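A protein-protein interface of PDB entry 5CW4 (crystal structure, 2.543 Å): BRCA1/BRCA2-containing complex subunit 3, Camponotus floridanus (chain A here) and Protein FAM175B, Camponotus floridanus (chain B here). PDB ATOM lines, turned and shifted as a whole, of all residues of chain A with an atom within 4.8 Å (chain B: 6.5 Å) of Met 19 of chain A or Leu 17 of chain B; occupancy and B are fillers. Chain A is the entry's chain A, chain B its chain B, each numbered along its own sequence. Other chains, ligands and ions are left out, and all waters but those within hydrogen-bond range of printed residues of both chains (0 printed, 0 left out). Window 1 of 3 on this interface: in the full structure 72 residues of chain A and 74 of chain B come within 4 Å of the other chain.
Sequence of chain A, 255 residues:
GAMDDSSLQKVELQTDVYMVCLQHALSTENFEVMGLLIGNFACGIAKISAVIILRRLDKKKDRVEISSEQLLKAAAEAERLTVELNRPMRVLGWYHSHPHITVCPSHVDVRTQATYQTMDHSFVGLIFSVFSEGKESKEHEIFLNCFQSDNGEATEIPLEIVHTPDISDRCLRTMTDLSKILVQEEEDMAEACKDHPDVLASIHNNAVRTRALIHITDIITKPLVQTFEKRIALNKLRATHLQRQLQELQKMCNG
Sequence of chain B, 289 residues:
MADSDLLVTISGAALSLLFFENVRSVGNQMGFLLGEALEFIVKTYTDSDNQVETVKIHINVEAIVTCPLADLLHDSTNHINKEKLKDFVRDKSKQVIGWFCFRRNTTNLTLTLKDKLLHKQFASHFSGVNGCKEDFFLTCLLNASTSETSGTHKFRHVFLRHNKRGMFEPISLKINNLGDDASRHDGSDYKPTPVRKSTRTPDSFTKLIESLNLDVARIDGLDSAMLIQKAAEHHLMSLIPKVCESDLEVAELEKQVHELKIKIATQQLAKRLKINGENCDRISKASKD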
ATOM      1  N   THR A  15      24.483  24.908  10.207  1.00  0.00           N
ATOM      2  CA  THR A  15      23.579  23.832   9.840  1.00  0.00           C
ATOM      3  C   THR A  15      24.153  22.890   8.777  1.00  0.00           C
ATOM      4  O   THR A  15      23.817  21.708   8.757  1.00  0.00           O
ATOM      5  CB  THR A  15      22.244  24.398   9.346  1.00  0.00           C
ATOM      6  OG1 THR A  15      22.494  25.453   8.411  1.00  0.00           O
ATOM      7  CG2 THR A  15      21.448  24.958  10.518  1.00  0.00           C
ATOM      8  N   ASP A  16      25.018  23.398   7.904  1.00  0.00           N
ATOM      9  CA  ASP A  16      25.594  22.555   6.854  1.00  0.00           C
ATOM     10  C   ASP A  16      26.696  21.654   7.412  1.00  0.00           C
ATOM     11  O   ASP A  16      26.910  20.549   6.920  1.00  0.00           O
ATOM     12  CB  ASP A  16      26.125  23.406   5.691  1.00  0.00           C
ATOM     13  CG  ASP A  16      27.181  24.409   6.124  1.00  0.00           C
ATOM     14  OD1 ASP A  16      27.373  24.595   7.346  1.00  0.00           O
ATOM     15  OD2 ASP A  16      27.810  25.025   5.234  1.00  0.00           O
ATOM     16  N   VAL A  17      27.391  22.130   8.441  1.00  0.00           N
ATOM     17  CA  VAL A  17      28.339  21.292   9.171  1.00  0.00           C
ATOM     18  C   VAL A  17      27.573  20.244   9.973  1.00  0.00           C
ATOM     19  O   VAL A  17      28.000  19.095  10.094  1.00  0.00           O
ATOM     20  CB  VAL A  17      29.235  22.123  10.113  1.00  0.00           C
ATOM     21  CG1 VAL A  17      29.966  21.220  11.105  1.00  0.00           C
ATOM     22  CG2 VAL A  17      30.218  22.949   9.306  1.00  0.00           C
ATOM     23  N   TYR A  18      26.434  20.659  10.516  1.00  0.00           N
ATOM     24  CA  TYR A  18      25.516  19.747  11.177  1.00  0.00           C
ATOM     25  C   TYR A  18      25.111  18.618  10.224  1.00  0.00           C
ATOM     26  O   TYR A  18      25.127  17.443  10.595  1.00  0.00           O
ATOM     27  CB  TYR A  18      24.283  20.510  11.678  1.00  0.00           C
ATOM     28  CG  TYR A  18      23.103  19.642  12.056  1.00  0.00           C
ATOM     29  CD1 TYR A  18      22.998  19.089  13.324  1.00  0.00           C
ATOM     30  CD2 TYR A  18      22.091  19.382  11.143  1.00  0.00           C
ATOM     31  CE1 TYR A  18      21.917  18.296  13.671  1.00  0.00           C
ATOM     32  CE2 TYR A  18      21.009  18.592  11.478  1.00  0.00           C
ATOM     33  CZ  TYR A  18      20.927  18.051  12.743  1.00  0.00           C
ATOM     34  OH  TYR A  18      19.852  17.265  13.081  1.00  0.00           O
ATOM     35  N   MET A  19      24.780  18.971   8.988  1.00  0.00           N
ATOM     36  CA  MET A  19      24.360  17.973   8.012  1.00  0.00           C
ATOM     37  C   MET A  19      25.466  16.967   7.712  1.00  0.00           C
ATOM     38  O   MET A  19      25.203  15.770   7.586  1.00  0.00           O
ATOM     39  CB  MET A  19      23.900  18.640   6.719  1.00  0.00           C
ATOM     40  CG  MET A  19      23.648  17.651   5.587  1.00  0.00           C
ATOM     41  SD  MET A  19      22.887  18.486   4.014  1.00  0.00           S
ATOM     42  CE  MET A  19      22.989  16.979   2.769  1.00  0.00           C
ATOM     43  N   VAL A  20      26.704  17.446   7.608  1.00  0.00           N
ATOM     44  CA  VAL A  20      27.832  16.565   7.310  1.00  0.00           C
ATOM     45  C   VAL A  20      28.049  15.524   8.408  1.00  0.00           C
ATOM     46  O   VAL A  20      28.162  14.332   8.120  1.00  0.00           O
ATOM     47  CB  VAL A  20      29.138  17.355   7.111  1.00  0.00           C
ATOM     48  CG1 VAL A  20      30.313  16.397   7.000  1.00  0.00           C
ATOM     49  CG2 VAL A  20      29.047  18.252   5.877  1.00  0.00           C
ATOM     50  N   CYS A  21      28.097  15.977   9.659  1.00  0.00           N
ATOM     51  CA  CYS A  21      28.303  15.078  10.794  1.00  0.00           C
ATOM     52  C   CYS A  21      27.199  14.035  10.895  1.00  0.00           C
ATOM     53  O   CYS A  21      27.469  12.834  10.981  1.00  0.00           O
ATOM     54  CB  CYS A  21      28.383  15.868  12.098  1.00  0.00           C
ATOM     55  SG  CYS A  21      29.714  17.092  12.142  1.00  0.00           S
ATOM     56  N   LEU A  22      25.955  14.508  10.882  1.00  0.00           N
ATOM     57  CA  LEU A  22      24.786  13.637  10.931  1.00  0.00           C
ATOM     58  C   LEU A  22      24.838  12.559   9.848  1.00  0.00           C
ATOM     59  O   LEU A  22      24.667  11.372  10.129  1.00  0.00           O
ATOM     60  CB  LEU A  22      23.511  14.468  10.790  1.00  0.00           C
ATOM     61  CG  LEU A  22      22.182  13.723  10.723  1.00  0.00           C
ATOM     62  CD1 LEU A  22      22.029  12.791  11.910  1.00  0.00           C
ATOM     63  CD2 LEU A  22      21.051  14.728  10.690  1.00  0.00           C
ATOM     64  N   GLN A  23      25.081  12.986   8.613  1.00  0.00           N
ATOM     65  CA  GLN A  23      25.229  12.070   7.488  1.00  0.00           C
ATOM     66  C   GLN A  23      26.318  11.039   7.763  1.00  0.00           C
ATOM     67  O   GLN A  23      26.169   9.854   7.467  1.00  0.00           O
ATOM     68  CB  GLN A  23      25.561  12.844   6.218  1.00  0.00           C
ATOM     69  CG  GLN A  23      25.557  12.013   4.946  1.00  0.00           C
ATOM     70  CD  GLN A  23      25.848  12.847   3.715  1.00  0.00           C
ATOM     71  OE1 GLN A  23      26.807  12.589   2.988  1.00  0.00           O
ATOM     72  NE2 GLN A  23      25.021  13.857   3.475  1.00  0.00           N
ATOM     73  N   ILE A 167      24.458  24.831   1.378  1.00  0.00           N
ATOM     74  CA  ILE A 167      25.467  23.865   1.797  1.00  0.00           C
ATOM     75  C   ILE A 167      26.780  24.271   1.142  1.00  0.00           C
ATOM     76  O   ILE A 167      26.937  24.140  -0.073  1.00  0.00           O
ATOM     77  CB  ILE A 167      25.102  22.429   1.396  1.00  0.00           C
ATOM     78  CG1 ILE A 167      23.602  22.184   1.580  1.00  0.00           C
ATOM     79  CG2 ILE A 167      25.923  21.428   2.194  1.00  0.00           C
ATOM     80  CD1 ILE A 167      23.114  20.877   0.972  1.00  0.00           C
ATOM     81  N   MET A 175      31.509  15.598   2.444  1.00  0.00           N
ATOM     82  CA  MET A 175      30.595  14.470   2.246  1.00  0.00           C
ATOM     83  C   MET A 175      31.150  13.478   1.229  1.00  0.00           C
ATOM     84  O   MET A 175      31.111  12.268   1.452  1.00  0.00           O
ATOM     85  CB  MET A 175      29.216  14.953   1.780  1.00  0.00           C
ATOM     86  CG  MET A 175      28.507  15.873   2.763  1.00  0.00           C
ATOM     87  SD  MET A 175      26.888  16.683   2.025  1.00  0.00           S
ATOM     88  CE  MET A 175      26.496  17.924   3.481  1.00  0.00           C
ATOM     89  N   THR A 227      21.065  12.572  -4.025  1.00  0.00           N
ATOM     90  CA  THR A 227      20.743  13.703  -3.165  1.00  0.00           C
ATOM     91  C   THR A 227      21.217  15.025  -3.763  1.00  0.00           C
ATOM     92  O   THR A 227      20.484  16.017  -3.741  1.00  0.00           O
ATOM     93  CB  THR A 227      21.349  13.527  -1.762  1.00  0.00           C
ATOM     94  OG1 THR A 227      20.633  12.501  -1.064  1.00  0.00           O
ATOM     95  CG2 THR A 227      21.256  14.817  -0.972  1.00  0.00           C
ATOM     96  N   ARG A 231      18.511  17.826  -5.328  1.00  0.00           N
ATOM     97  CA  ARG A 231      18.560  19.128  -4.676  1.00  0.00           C
ATOM     98  C   ARG A 231      18.564  20.214  -5.742  1.00  0.00           C
ATOM     99  O   ARG A 231      17.824  21.198  -5.659  1.00  0.00           O
ATOM    100  CB  ARG A 231      19.801  19.233  -3.783  1.00  0.00           C
ATOM    101  CG  ARG A 231      19.851  20.458  -2.873  1.00  0.00           C
ATOM    102  CD  ARG A 231      18.599  20.537  -2.002  1.00  0.00           C
ATOM    103  NE  ARG A 231      18.710  21.333  -0.774  1.00  0.00           N
ATOM    104  CZ  ARG A 231      19.606  22.286  -0.524  1.00  0.00           C
ATOM    105  NH1 ARG A 231      20.527  22.625  -1.415  1.00  0.00           N
ATOM    106  NH2 ARG A 231      19.569  22.916   0.638  1.00  0.00           N
ATOM    107  N   GLY B  12      21.106   7.686   4.542  1.00  0.00           N
ATOM    108  CA  GLY B  12      21.665   8.672   5.441  1.00  0.00           C
ATOM    109  C   GLY B  12      21.754  10.017   4.751  1.00  0.00           C
ATOM    110  O   GLY B  12      21.552  11.056   5.381  1.00  0.00           O
ATOM    111  N   ALA B  13      22.049   9.994   3.452  1.00  0.00           N
ATOM    112  CA  ALA B  13      22.161  11.220   2.660  1.00  0.00           C
ATOM    113  C   ALA B  13      20.842  11.979   2.634  1.00  0.00           C
ATOM    114  O   ALA B  13      20.795  13.169   2.936  1.00  0.00           O
ATOM    115  CB  ALA B  13      22.610  10.901   1.240  1.00  0.00           C
ATOM    116  N   ALA B  14      19.769  11.282   2.273  1.00  0.00           N
ATOM    117  CA  ALA B  14      18.456  11.901   2.180  1.00  0.00           C
ATOM    118  C   ALA B  14      17.976  12.414   3.536  1.00  0.00           C
ATOM    119  O   ALA B  14      17.508  13.548   3.645  1.00  0.00           O
ATOM    120  CB  ALA B  14      17.447  10.918   1.599  1.00  0.00           C
ATOM    121  N   LEU B  15      18.094  11.581   4.566  1.00  0.00           N
ATOM    122  CA  LEU B  15      17.632  11.956   5.896  1.00  0.00           C
ATOM    123  C   LEU B  15      18.393  13.176   6.418  1.00  0.00           C
ATOM    124  O   LEU B  15      17.808  14.059   7.047  1.00  0.00           O
ATOM    125  CB  LEU B  15      17.772  10.784   6.873  1.00  0.00           C
ATOM    126  CG  LEU B  15      17.149  11.004   8.257  1.00  0.00           C
ATOM    127  CD1 LEU B  15      15.696  11.413   8.121  1.00  0.00           C
ATOM    128  CD2 LEU B  15      17.263   9.764   9.127  1.00  0.00           C
ATOM    129  N   SER B  16      19.694  13.231   6.146  1.00  0.00           N
ATOM    130  CA  SER B  16      20.510  14.338   6.628  1.00  0.00           C
ATOM    131  C   SER B  16      20.095  15.634   5.944  1.00  0.00           C
ATOM    132  O   SER B  16      20.139  16.707   6.549  1.00  0.00           O
ATOM    133  CB  SER B  16      22.001  14.065   6.396  1.00  0.00           C
ATOM    134  OG  SER B  16      22.348  14.246   5.033  1.00  0.00           O
ATOM    135  N   LEU B  17      19.688  15.531   4.682  1.00  0.00           N
ATOM    136  CA  LEU B  17      19.193  16.693   3.950  1.00  0.00           C
ATOM    137  C   LEU B  17      17.862  17.178   4.521  1.00  0.00           C
ATOM    138  O   LEU B  17      17.627  18.382   4.633  1.00  0.00           O
ATOM    139  CB  LEU B  17      19.032  16.379   2.467  1.00  0.00           C
ATOM    140  CG  LEU B  17      18.516  17.554   1.629  1.00  0.00           C
ATOM    141  CD1 LEU B  17      19.425  18.756   1.800  1.00  0.00           C
ATOM    142  CD2 LEU B  17      18.427  17.168   0.167  1.00  0.00           C
ATOM    143  N   LEU B  18      16.992  16.235   4.872  1.00  0.00           N
ATOM    144  CA  LEU B  18      15.718  16.568   5.498  1.00  0.00           C
ATOM    145  C   LEU B  18      15.953  17.344   6.790  1.00  0.00           C
ATOM    146  O   LEU B  18      15.394  18.422   6.985  1.00  0.00           O
ATOM    147  CB  LEU B  18      14.897  15.301   5.773  1.00  0.00           C
ATOM    148  CG  LEU B  18      13.516  15.475   6.421  1.00  0.00           C
ATOM    149  CD1 LEU B  18      12.700  16.569   5.734  1.00  0.00           C
ATOM    150  CD2 LEU B  18      12.746  14.158   6.404  1.00  0.00           C
ATOM    151  N   PHE B  19      16.793  16.794   7.664  1.00  0.00           N
ATOM    152  CA  PHE B  19      17.122  17.443   8.929  1.00  0.00           C
ATOM    153  C   PHE B  19      17.787  18.803   8.723  1.00  0.00           C
ATOM    154  O   PHE B  19      17.470  19.769   9.422  1.00  0.00           O
ATOM    155  CB  PHE B  19      18.019  16.538   9.769  1.00  0.00           C
ATOM    156  CG  PHE B  19      17.265  15.488  10.526  1.00  0.00           C
ATOM    157  CD1 PHE B  19      16.395  14.635   9.869  1.00  0.00           C
ATOM    158  CD2 PHE B  19      17.419  15.354  11.891  1.00  0.00           C
ATOM    159  CE1 PHE B  19      15.691  13.665  10.560  1.00  0.00           C
ATOM    160  CE2 PHE B  19      16.723  14.386  12.588  1.00  0.00           C
ATOM    161  CZ  PHE B  19      15.856  13.539  11.919  1.00  0.00           C
ATOM    162  N   PHE B  20      18.709  18.871   7.767  1.00  0.00           N
ATOM    163  CA  PHE B  20      19.332  20.132   7.382  1.00  0.00           C
ATOM    164  C   PHE B  20      18.277  21.191   7.088  1.00  0.00           C
ATOM    165  O   PHE B  20      18.278  22.269   7.681  1.00  0.00           O
ATOM    166  CB  PHE B  20      20.230  19.924   6.163  1.00  0.00           C
ATOM    167  CG  PHE B  20      20.715  21.205   5.526  1.00  0.00           C
ATOM    168  CD1 PHE B  20      21.589  22.049   6.199  1.00  0.00           C
ATOM    169  CD2 PHE B  20      20.325  21.542   4.237  1.00  0.00           C
ATOM    170  CE1 PHE B  20      22.047  23.218   5.606  1.00  0.00           C
ATOM    171  CE2 PHE B  20      20.783  22.712   3.638  1.00  0.00           C
ATOM    172  CZ  PHE B  20      21.646  23.548   4.322  1.00  0.00           C
ATOM    173  N   GLU B  21      17.367  20.860   6.177  1.00  0.00           N
ATOM    174  CA  GLU B  21      16.300  21.764   5.774  1.00  0.00           C
ATOM    175  C   GLU B  21      15.426  22.167   6.968  1.00  0.00           C
ATOM    176  O   GLU B  21      15.002  23.319   7.074  1.00  0.00           O
ATOM    177  CB  GLU B  21      15.455  21.111   4.678  1.00  0.00           C
ATOM    178  CG  GLU B  21      14.827  22.089   3.704  1.00  0.00           C
ATOM    179  CD  GLU B  21      15.841  22.769   2.796  1.00  0.00           C
ATOM    180  OE1 GLU B  21      15.453  23.724   2.088  1.00  0.00           O
ATOM    181  OE2 GLU B  21      17.018  22.351   2.785  1.00  0.00           O
ATOM    182  N   ASN B  22      15.175  21.221   7.872  1.00  0.00           N
ATOM    183  CA  ASN B  22      14.393  21.500   9.075  1.00  0.00           C
ATOM    184  C   ASN B  22      15.068  22.506  10.006  1.00  0.00           C
ATOM    185  O   ASN B  22      14.458  23.497  10.402  1.00  0.00           O
ATOM    186  CB  ASN B  22      14.113  20.207   9.852  1.00  0.00           C
ATOM    187  CG  ASN B  22      13.081  19.318   9.175  1.00  0.00           C
ATOM    188  OD1 ASN B  22      12.361  19.747   8.267  1.00  0.00           O
ATOM    189  ND2 ASN B  22      12.992  18.071   9.632  1.00  0.00           N
ATOM    190  N   ARG B  24      17.404  24.572   9.424  1.00  0.00           N
ATOM    191  CA  ARG B  24      17.567  25.860   8.743  1.00  0.00           C
ATOM    192  C   ARG B  24      16.373  26.781   8.940  1.00  0.00           C
ATOM    193  O   ARG B  24      16.527  27.996   9.047  1.00  0.00           O
ATOM    194  CB  ARG B  24      17.750  25.671   7.241  1.00  0.00           C
ATOM    195  CG  ARG B  24      19.054  25.085   6.789  1.00  0.00           C
ATOM    196  CD  ARG B  24      18.976  24.856   5.293  1.00  0.00           C
ATOM    197  NE  ARG B  24      18.505  26.045   4.586  1.00  0.00           N
ATOM    198  CZ  ARG B  24      18.099  26.054   3.321  1.00  0.00           C
ATOM    199  NH1 ARG B  24      18.094  24.932   2.615  1.00  0.00           N
ATOM    200  NH2 ARG B  24      17.688  27.184   2.765  1.00  0.00           N
ATOM    201  N   ALA B  63      14.261  11.837  -1.833  1.00  0.00           N
ATOM    202  CA  ALA B  63      14.483  13.274  -1.764  1.00  0.00           C
ATOM    203  C   ALA B  63      13.287  13.999  -1.167  1.00  0.00           C
ATOM    204  O   ALA B  63      12.196  13.439  -1.056  1.00  0.00           O
ATOM    205  CB  ALA B  63      14.792  13.825  -3.140  1.00  0.00           C
ATOM    206  N   ILE B  64      13.499  15.253  -0.787  1.00  0.00           N
ATOM    207  CA  ILE B  64      12.441  16.050  -0.188  1.00  0.00           C
ATOM    208  C   ILE B  64      12.495  17.486  -0.694  1.00  0.00           C
ATOM    209  O   ILE B  64      13.548  17.965  -1.113  1.00  0.00           O
ATOM    210  CB  ILE B  64      12.528  16.036   1.357  1.00  0.00           C
ATOM    211  CG1 ILE B  64      13.768  16.792   1.844  1.00  0.00           C
ATOM    212  CG2 ILE B  64      12.524  14.616   1.870  1.00  0.00           C
ATOM    213  CD1 ILE B  64      13.524  18.271   2.122  1.00  0.00           C
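The guanidinium group (NH1) of Arg 24 of chain B sits close to the guanidinium group (NH2) of Arg 231 of chain A. The guanidinium group of Arg 231 of chain A is in salt-bridge range of the side-chain carboxylate of Glu 21 of chain B (3.4 Å). The side-chain hydroxyl of Ser 16 of chain B lies within hydrogen-bond range of the side-chain amide nitrogen of Gln 23 of chain A (3.1 Å).
Printed residues of chain B that touch a printed residue of chain A: Ala 13, Ala 14, Ser 16, Leu 17, Phe 19, Phe 20, Glu 21 and Arg 24. Hydrophobic or aromatic side chains of chain A that line the printed part of chain B: Tyr 18, Met 19, Leu 22 and Ile 167. Among the printed residues, Asp or Glu carboxylates within 4 Å of a Lys or Arg side-chain nitrogen of the other chain: Arg 231 of chain A with Glu 21 of chain B (3.4 Å).
OE2 of Glu 21 of chain B is in salt-bridge range of NH1 of Arg 24 of chain B (2.8 Å). O of Gly 12 of chain B sits close to OG of Ser 16 of chain B, at 3.3 Å. The backbone carbonyl oxygen of Ala 13 of chain B lies within hydrogen-bond range of the side-chain hydroxyl of Ser 16 of chain B, at 2.8 Å. NE2 of Gln 23 of chain A lies within hydrogen-bond range of SD of Met 175 of chain A.
Of the printed residues of chain B, Asp 16 of chain A touches Phe 20 (3.8 Å). Of the printed residues of chain B, Met 19 of chain A touches Ser 16 (3.6 Å), Leu 17 (3.99 Å) and Phe 20 (3.7 Å). Printed residues of chain B within 4 Å of Gln 23 of chain A: Ala 13 (3.97 Å) and Ser 16 (3.1 Å). Met 175 of chain A touches none of the printed residues of chain B. Of the printed residues of chain A, Ala 13 of chain B touches Gln 23 and Thr 227. Of the printed residues of chain A, Phe 19 of chain B touches Tyr 18 and Leu 22. Printed residues of chain A within 4 Å of Glu 21 of chain B: Arg 231 (3.4 Å). The nearest printed residue of chain B that does not touch Met 19 of chain A is Ala 13 of chain B (4.4 Å).
Among the printed residues, pairs that only touch across the chains: Thr 15 of chain A with Phe 20 of chain B (3.4 Å), Thr 15 of chain A with Arg 24 of chain B (3.8 Å), Asp 16 of chain A with Phe 20 of chain B (3.8 Å), Tyr 18 of chain A with Phe 19 of chain B (3.3 Å), Met 19 of chain A with Ser 16 of chain B (3.6 Å), Met 19 of chain A with Leu 17 of chain B (3.99 Å), Met 19 of chain A with Phe 20 of chain B (3.7 Å), Leu 22 of chain A with Phe 19 of chain B (3.6 Å), Gln 23 of chain A with Ala 13 of chain B (3.97 Å), Ile 167 of chain A with Phe 20 of chain B (3.5 Å), Thr 227 of chain A with Ala 13 of chain B (3.4 Å), Thr 227 of chain A with Ala 14 of chain B (3.7 Å), Thr 227 of chain A with Leu 17 of chain B (3.9 Å), Arg 231 of chain A with Leu 17 of chain B (3.7 Å) and Arg 231 of chain A with Phe 20 of chain B (3.2 Å).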
